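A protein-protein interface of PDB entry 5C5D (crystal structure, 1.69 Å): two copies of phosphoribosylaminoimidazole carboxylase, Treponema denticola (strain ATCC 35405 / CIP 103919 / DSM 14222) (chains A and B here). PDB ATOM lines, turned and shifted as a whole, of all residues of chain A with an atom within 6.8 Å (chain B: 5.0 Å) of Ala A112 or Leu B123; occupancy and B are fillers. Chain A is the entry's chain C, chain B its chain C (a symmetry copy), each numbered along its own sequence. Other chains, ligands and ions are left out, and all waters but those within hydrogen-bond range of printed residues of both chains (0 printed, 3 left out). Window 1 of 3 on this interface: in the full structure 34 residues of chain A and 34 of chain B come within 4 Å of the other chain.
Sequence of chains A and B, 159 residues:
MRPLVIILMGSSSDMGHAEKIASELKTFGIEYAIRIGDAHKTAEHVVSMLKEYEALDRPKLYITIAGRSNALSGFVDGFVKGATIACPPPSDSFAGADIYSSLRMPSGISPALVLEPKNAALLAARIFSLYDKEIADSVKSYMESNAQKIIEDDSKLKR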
ATOM      1  N   ASP A  77      17.191 -25.590 -17.517  1.00  0.00           N
ATOM      2  CA  ASP A  77      17.149 -25.395 -18.947  1.00  0.00           C
ATOM      3  C   ASP A  77      15.725 -25.507 -19.537  1.00  0.00           C
ATOM      4  O   ASP A  77      15.377 -24.803 -20.485  1.00  0.00           O
ATOM      5  CB  ASP A  77      18.082 -26.385 -19.632  1.00  0.00           C
ATOM      6  CG  ASP A  77      18.332 -26.025 -21.066  1.00  0.00           C
ATOM      7  OD1 ASP A  77      19.190 -25.140 -21.319  1.00  0.00           O
ATOM      8  OD2 ASP A  77      17.645 -26.565 -21.952  1.00  0.00           O
ATOM      9  N   ALA A  83      19.828 -19.411 -23.113  1.00  0.00           N
ATOM     10  CA  ALA A  83      20.806 -20.491 -22.982  1.00  0.00           C
ATOM     11  C   ALA A  83      21.269 -20.722 -21.561  1.00  0.00           C
ATOM     12  O   ALA A  83      21.228 -19.840 -20.691  1.00  0.00           O
ATOM     13  CB  ALA A  83      21.991 -20.184 -23.877  1.00  0.00           C
ATOM     14  N   THR A  84      21.663 -21.965 -21.321  1.00  0.00           N
ATOM     15  CA  THR A  84      22.263 -22.388 -20.066  1.00  0.00           C
ATOM     16  C   THR A  84      23.474 -23.279 -20.338  1.00  0.00           C
ATOM     17  O   THR A  84      23.653 -23.832 -21.435  1.00  0.00           O
ATOM     18  CB  THR A  84      21.283 -23.150 -19.137  1.00  0.00           C
ATOM     19  OG1 THR A  84      21.128 -24.521 -19.552  1.00  0.00           O
ATOM     20  CG2 THR A  84      19.916 -22.495 -19.090  1.00  0.00           C
ATOM     21  N   ILE A  85      24.314 -23.344 -19.315  1.00  0.00           N
ATOM     22  CA  ILE A  85      25.577 -24.070 -19.300  1.00  0.00           C
ATOM     23  C   ILE A  85      25.598 -24.987 -18.093  1.00  0.00           C
ATOM     24  O   ILE A  85      25.394 -24.542 -16.978  1.00  0.00           O
ATOM     25  CB  ILE A  85      26.762 -23.100 -19.230  1.00  0.00           C
ATOM     26  CG1 ILE A  85      26.794 -22.171 -20.450  1.00  0.00           C
ATOM     27  CG2 ILE A  85      28.094 -23.883 -19.071  1.00  0.00           C
ATOM     28  CD1 ILE A  85      27.664 -20.984 -20.270  1.00  0.00           C
ATOM     29  N   ALA A  86      25.860 -26.269 -18.330  1.00  0.00           N
ATOM     30  CA  ALA A  86      26.040 -27.267 -17.280  1.00  0.00           C
ATOM     31  C   ALA A  86      27.540 -27.398 -17.024  1.00  0.00           C
ATOM     32  O   ALA A  86      28.339 -27.583 -17.947  1.00  0.00           O
ATOM     33  CB  ALA A  86      25.440 -28.611 -17.705  1.00  0.00           C
ATOM     34  N   CYS A  87      27.923 -27.275 -15.754  1.00  0.00           N
ATOM     35  CA  CYS A  87      29.333 -27.396 -15.366  1.00  0.00           C
ATOM     36  C   CYS A  87      29.363 -28.208 -14.059  1.00  0.00           C
ATOM     37  O   CYS A  87      29.442 -27.671 -12.967  1.00  0.00           O
ATOM     38  CB  CYS A  87      29.944 -26.036 -15.206  1.00  0.00           C
ATOM     39  SG  CYS A  87      31.774 -26.233 -14.995  1.00  0.00           S
ATOM     40  N   SER A 110      18.635 -28.314 -23.847  1.00  0.00           N
ATOM     41  CA  SER A 110      19.884 -28.066 -24.537  1.00  0.00           C
ATOM     42  C   SER A 110      20.952 -27.323 -23.766  1.00  0.00           C
ATOM     43  O   SER A 110      21.567 -26.411 -24.332  1.00  0.00           O
ATOM     44  CB  SER A 110      19.594 -27.274 -25.826  1.00  0.00           C
ATOM     45  OG  SER A 110      19.106 -25.988 -25.486  1.00  0.00           O
ATOM     46  N   PRO A 111      21.234 -27.707 -22.510  1.00  0.00           N
ATOM     47  CA  PRO A 111      22.337 -27.035 -21.815  1.00  0.00           C
ATOM     48  C   PRO A 111      23.676 -27.325 -22.486  1.00  0.00           C
ATOM     49  O   PRO A 111      23.916 -28.432 -22.965  1.00  0.00           O
ATOM     50  CB  PRO A 111      22.276 -27.629 -20.418  1.00  0.00           C
ATOM     51  CG  PRO A 111      21.610 -28.921 -20.596  1.00  0.00           C
ATOM     52  CD  PRO A 111      20.644 -28.759 -21.664  1.00  0.00           C
ATOM     53  N   ALA A 112      24.538 -26.332 -22.530  1.00  0.00           N
ATOM     54  CA  ALA A 112      25.893 -26.487 -23.011  1.00  0.00           C
ATOM     55  C   ALA A 112      26.740 -27.181 -21.936  1.00  0.00           C
ATOM     56  O   ALA A 112      26.904 -26.631 -20.848  1.00  0.00           O
ATOM     57  CB  ALA A 112      26.477 -25.146 -23.319  1.00  0.00           C
ATOM     58  N   LEU A 113      27.323 -28.338 -22.226  1.00  0.00           N
ATOM     59  CA  LEU A 113      28.147 -28.994 -21.203  1.00  0.00           C
ATOM     60  C   LEU A 113      29.596 -28.569 -21.389  1.00  0.00           C
ATOM     61  O   LEU A 113      30.135 -28.660 -22.511  1.00  0.00           O
ATOM     62  CB  LEU A 113      28.042 -30.501 -21.304  1.00  0.00           C
ATOM     63  CG  LEU A 113      28.859 -31.392 -20.356  1.00  0.00           C
ATOM     64  CD1 LEU A 113      28.524 -31.051 -18.903  1.00  0.00           C
ATOM     65  CD2 LEU A 113      28.521 -32.812 -20.686  1.00  0.00           C
ATOM     66  N   VAL A 114      30.198 -28.140 -20.278  1.00  0.00           N
ATOM     67  CA  VAL A 114      31.614 -27.798 -20.217  1.00  0.00           C
ATOM     68  C   VAL A 114      32.160 -28.367 -18.907  1.00  0.00           C
ATOM     69  O   VAL A 114      31.532 -28.204 -17.863  1.00  0.00           O
ATOM     70  CB  VAL A 114      31.822 -26.297 -20.252  1.00  0.00           C
ATOM     71  CG1 VAL A 114      33.286 -25.957 -20.187  1.00  0.00           C
ATOM     72  CG2 VAL A 114      31.223 -25.678 -21.526  1.00  0.00           C
ATOM     73  N   LEU A 123      33.178 -19.762 -21.913  1.00  0.00           N
ATOM     74  CA  LEU A 123      32.058 -19.959 -22.835  1.00  0.00           C
ATOM     75  C   LEU A 123      30.978 -18.875 -22.604  1.00  0.00           C
ATOM     76  O   LEU A 123      30.470 -18.292 -23.567  1.00  0.00           O
ATOM     77  CB  LEU A 123      31.478 -21.364 -22.676  1.00  0.00           C
ATOM     78  CG  LEU A 123      30.184 -21.582 -23.463  1.00  0.00           C
ATOM     79  CD1 LEU A 123      30.382 -21.478 -24.949  1.00  0.00           C
ATOM     80  CD2 LEU A 123      29.617 -22.953 -23.070  1.00  0.00           C
ATOM     81  N   ILE A 127      29.753 -16.256 -25.371  1.00  0.00           N
ATOM     82  CA  ILE A 127      28.344 -16.145 -25.743  1.00  0.00           C
ATOM     83  C   ILE A 127      27.902 -14.683 -25.765  1.00  0.00           C
ATOM     84  O   ILE A 127      27.309 -14.199 -26.757  1.00  0.00           O
ATOM     85  CB  ILE A 127      27.472 -16.948 -24.789  1.00  0.00           C
ATOM     86  CG1 ILE A 127      27.564 -18.420 -25.157  1.00  0.00           C
ATOM     87  CG2 ILE A 127      25.987 -16.500 -24.858  1.00  0.00           C
ATOM     88  CD1 ILE A 127      26.944 -19.389 -24.181  1.00  0.00           C
ATOM     89  N   ILE B  85      30.124 -24.583 -30.601  1.00  0.00           N
ATOM     90  CA  ILE B  85      29.366 -25.743 -30.149  1.00  0.00           C
ATOM     91  C   ILE B  85      29.922 -26.982 -30.822  1.00  0.00           C
ATOM     92  O   ILE B  85      30.021 -27.032 -32.035  1.00  0.00           O
ATOM     93  CB  ILE B  85      27.880 -25.590 -30.498  1.00  0.00           C
ATOM     94  CG1 ILE B  85      27.271 -24.361 -29.812  1.00  0.00           C
ATOM     95  CG2 ILE B  85      27.105 -26.889 -30.141  1.00  0.00           C
ATOM     96  CD1 ILE B  85      25.971 -23.942 -30.389  1.00  0.00           C
ATOM     97  N   ALA B 112      30.964 -25.571 -26.402  1.00  0.00           N
ATOM     98  CA  ALA B 112      29.797 -26.120 -25.747  1.00  0.00           C
ATOM     99  C   ALA B 112      29.512 -27.520 -26.303  1.00  0.00           C
ATOM    100  O   ALA B 112      29.236 -27.652 -27.494  1.00  0.00           O
ATOM    101  CB  ALA B 112      28.618 -25.235 -25.990  1.00  0.00           C
ATOM    102  N   LEU B 113      29.515 -28.555 -25.471  1.00  0.00           N
ATOM    103  CA  LEU B 113      29.224 -29.893 -26.000  1.00  0.00           C
ATOM    104  C   LEU B 113      27.737 -30.171 -25.850  1.00  0.00           C
ATOM    105  O   LEU B 113      27.177 -30.005 -24.746  1.00  0.00           O
ATOM    106  CB  LEU B 113      30.017 -30.953 -25.263  1.00  0.00           C
ATOM    107  CG  LEU B 113      29.835 -32.435 -25.623  1.00  0.00           C
ATOM    108  CD1 LEU B 113      30.136 -32.651 -27.108  1.00  0.00           C
ATOM    109  CD2 LEU B 113      30.762 -33.218 -24.748  1.00  0.00           C
ATOM    110  N   VAL B 114      27.138 -30.613 -26.957  1.00  0.00           N
ATOM    111  CA  VAL B 114      25.746 -31.046 -26.996  1.00  0.00           C
ATOM    112  C   VAL B 114      25.692 -32.313 -27.852  1.00  0.00           C
ATOM    113  O   VAL B 114      26.285 -32.348 -28.927  1.00  0.00           O
ATOM    114  CB  VAL B 114      24.851 -29.981 -27.597  1.00  0.00           C
ATOM    115  CG1 VAL B 114      23.419 -30.441 -27.632  1.00  0.00           C
ATOM    116  CG2 VAL B 114      24.933 -28.668 -26.801  1.00  0.00           C
ATOM    117  N   ASN B 119      19.393 -30.446 -30.467  1.00  0.00           N
ATOM    118  CA  ASN B 119      19.733 -29.641 -29.293  1.00  0.00           C
ATOM    119  C   ASN B 119      20.884 -28.704 -29.625  1.00  0.00           C
ATOM    120  O   ASN B 119      20.951 -27.626 -29.048  1.00  0.00           O
ATOM    121  CB  ASN B 119      20.086 -30.508 -28.083  1.00  0.00           C
ATOM    122  CG  ASN B 119      18.861 -31.083 -27.421  1.00  0.00           C
ATOM    123  OD1 ASN B 119      17.754 -30.577 -27.616  1.00  0.00           O
ATOM    124  ND2 ASN B 119      19.034 -32.173 -26.662  1.00  0.00           N
ATOM    125  N   ALA B 120      21.776 -29.079 -30.544  1.00  0.00           N
ATOM    126  CA  ALA B 120      22.822 -28.147 -30.960  1.00  0.00           C
ATOM    127  C   ALA B 120      22.163 -26.933 -31.609  1.00  0.00           C
ATOM    128  O   ALA B 120      22.544 -25.776 -31.368  1.00  0.00           O
ATOM    129  CB  ALA B 120      23.778 -28.792 -31.939  1.00  0.00           C
ATOM    130  N   ALA B 121      21.176 -27.177 -32.467  1.00  0.00           N
ATOM    131  CA  ALA B 121      20.446 -26.087 -33.095  1.00  0.00           C
ATOM    132  C   ALA B 121      19.695 -25.232 -32.057  1.00  0.00           C
ATOM    133  O   ALA B 121      19.708 -24.000 -32.131  1.00  0.00           O
ATOM    134  CB  ALA B 121      19.469 -26.605 -34.144  1.00  0.00           C
ATOM    135  N   LEU B 122      19.017 -25.870 -31.109  1.00  0.00           N
ATOM    136  CA  LEU B 122      18.282 -25.139 -30.071  1.00  0.00           C
ATOM    137  C   LEU B 122      19.240 -24.318 -29.192  1.00  0.00           C
ATOM    138  O   LEU B 122      18.938 -23.156 -28.887  1.00  0.00           O
ATOM    139  CB  LEU B 122      17.475 -26.099 -29.199  1.00  0.00           C
ATOM    140  CG  LEU B 122      16.666 -25.488 -28.054  1.00  0.00           C
ATOM    141  CD1 LEU B 122      15.633 -24.499 -28.563  1.00  0.00           C
ATOM    142  CD2 LEU B 122      15.988 -26.617 -27.259  1.00  0.00           C
ATOM    143  N   LEU B 123      20.385 -24.895 -28.813  1.00  0.00           N
ATOM    144  CA  LEU B 123      21.348 -24.114 -28.036  1.00  0.00           C
ATOM    145  C   LEU B 123      21.807 -22.874 -28.842  1.00  0.00           C
ATOM    146  O   LEU B 123      21.862 -21.767 -28.297  1.00  0.00           O
ATOM    147  CB  LEU B 123      22.537 -24.984 -27.632  1.00  0.00           C
ATOM    148  CG  LEU B 123      23.679 -24.195 -26.985  1.00  0.00           C
ATOM    149  CD1 LEU B 123      23.283 -23.560 -25.683  1.00  0.00           C
ATOM    150  CD2 LEU B 123      24.868 -25.149 -26.803  1.00  0.00           C
ATOM    151  N   ALA B 124      22.148 -23.071 -30.109  1.00  0.00           N
ATOM    152  CA  ALA B 124      22.518 -21.948 -30.977  1.00  0.00           C
ATOM    153  C   ALA B 124      21.438 -20.878 -30.975  1.00  0.00           C
ATOM    154  O   ALA B 124      21.730 -19.689 -30.779  1.00  0.00           O
ATOM    155  CB  ALA B 124      22.806 -22.452 -32.403  1.00  0.00           C
ATOM    156  N   ALA B 125      20.178 -21.270 -31.178  1.00  0.00           N
ATOM    157  CA  ALA B 125      19.077 -20.305 -31.161  1.00  0.00           C
ATOM    158  C   ALA B 125      19.010 -19.578 -29.829  1.00  0.00           C
ATOM    159  O   ALA B 125      18.791 -18.359 -29.774  1.00  0.00           O
ATOM    160  CB  ALA B 125      17.767 -21.017 -31.446  1.00  0.00           C
ATOM    161  N   ARG B 126      19.166 -20.324 -28.735  1.00  0.00           N
ATOM    162  CA  ARG B 126      19.006 -19.729 -27.415  1.00  0.00           C
ATOM    163  C   ARG B 126      20.167 -18.808 -27.066  1.00  0.00           C
ATOM    164  O   ARG B 126      20.015 -17.867 -26.289  1.00  0.00           O
ATOM    165  CB  ARG B 126      18.820 -20.837 -26.394  1.00  0.00           C
ATOM    166  CG  ARG B 126      17.448 -21.459 -26.626  1.00  0.00           C
ATOM    167  CD  ARG B 126      17.225 -22.677 -25.754  1.00  0.00           C
ATOM    168  NE  ARG B 126      16.976 -22.310 -24.364  1.00  0.00           N
ATOM    169  CZ  ARG B 126      16.817 -23.208 -23.403  1.00  0.00           C
ATOM    170  NH1 ARG B 126      16.920 -24.490 -23.702  1.00  0.00           N
ATOM    171  NH2 ARG B 126      16.563 -22.837 -22.159  1.00  0.00           N
ATOM    172  N   ILE B 127      21.316 -19.082 -27.662  1.00  0.00           N
ATOM    173  CA  ILE B 127      22.451 -18.168 -27.544  1.00  0.00           C
ATOM    174  C   ILE B 127      22.143 -16.831 -28.215  1.00  0.00           C
ATOM    175  O   ILE B 127      22.317 -15.747 -27.612  1.00  0.00           O
ATOM    176  CB  ILE B 127      23.703 -18.788 -28.146  1.00  0.00           C
ATOM    177  CG1 ILE B 127      24.275 -19.797 -27.164  1.00  0.00           C
ATOM    178  CG2 ILE B 127      24.781 -17.714 -28.454  1.00  0.00           C
ATOM    179  CD1 ILE B 127      25.389 -20.672 -27.683  1.00  0.00           C
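The guanidinium group (NH1) of Arg B126 lies within salt-bridge range of the side-chain carboxylate (OD2) of Asp A77 (2.8 Å). OG of Ser A110 sits at hydrogen-bond distance from NH1 of Arg B126 (3.2 Å). The backbone carbonyl oxygen (O) of Leu A113 is in hydrogen-bond range of the backbone NH (N) of Leu B113.
Among the printed residues, pairs that only touch across the chains: Ala A83 with Arg B126, Ala A83 with Ile B127, Ser A110 with Asn B119, Ser A110 with Leu B122, Ser A110 with Leu B123, Pro A111 with Val B114, Ala A112 with Ala B112, Ala A112 with Leu B123, Leu A123 with Ala B112 and Ile A127 with Ile B127.
Ala B112 touches its own counterpart, Ala A112. Ala A112 touches Leu B123, and with the chains exchanged Leu A123 touches Ala B112. Leu A113 touches its own counterpart, Leu B113. Ile A127 touches its own counterpart, Ile B127. Positions printed for both chains: 85, 112, 113, 114, 123 and 127. Of the 13 pairs that touch across the chains among the printed residues, 5 have their exchanged pair printed and touching as well.
The side-chain carboxylate of Asp A77 sits at hydrogen-bond distance from the side-chain hydroxyl of Thr A84 (2.7 Å). The side-chain carboxylate of Asp A77 lies within hydrogen-bond range of the backbone NH of Ser A110, at 2.8 Å. The backbone carbonyl oxygen (O) of Thr A84 lies within hydrogen-bond range of the backbone NH (N) of Ala A112 (2.9 Å). N of Ala A86 sits at hydrogen-bond distance from O of Ala A112 (2.7 Å).
Of the 13 printed residues of chain A, 8 touch a printed residue of chain B. Hydrophobic or aromatic side chains of chain A that line the printed part of chain B: Ala A83, Ala A112, Leu A113, Leu A123 and Ile A127. Among the printed residues, 13 pairs touch across the chains. Among the printed residues, Asp or Glu carboxylates within 4 Å of a Lys or Arg side-chain nitrogen of the other chain: Asp A77 with Arg B126 (2.8 Å).
Of the printed residues of chain B, Ala A112 touches Ala B112 (3.4 Å) and Leu B123 (3.8 Å). Leu B123 touches just these residues of chain A: Ser A110 (3.6 Å) and Ala A112 (3.8 Å). Printed residues of chain A within 4 Å of Ala B112: Ala A112 and Leu A123. Printed residues of chain A within 4 Å of Asn B119: Ser A110 (3.5 Å). Of the printed residues of chain B, Ser A110 touches Asn B119, Leu B122, Leu B123 and Arg B126. Ile A85 touches none of the printed residues of chain B. Ala B125 touches none of the printed residues of chain A. The nearest printed residue of chain A that does not touch Ala B112 is Leu A113 (4.01 Å).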
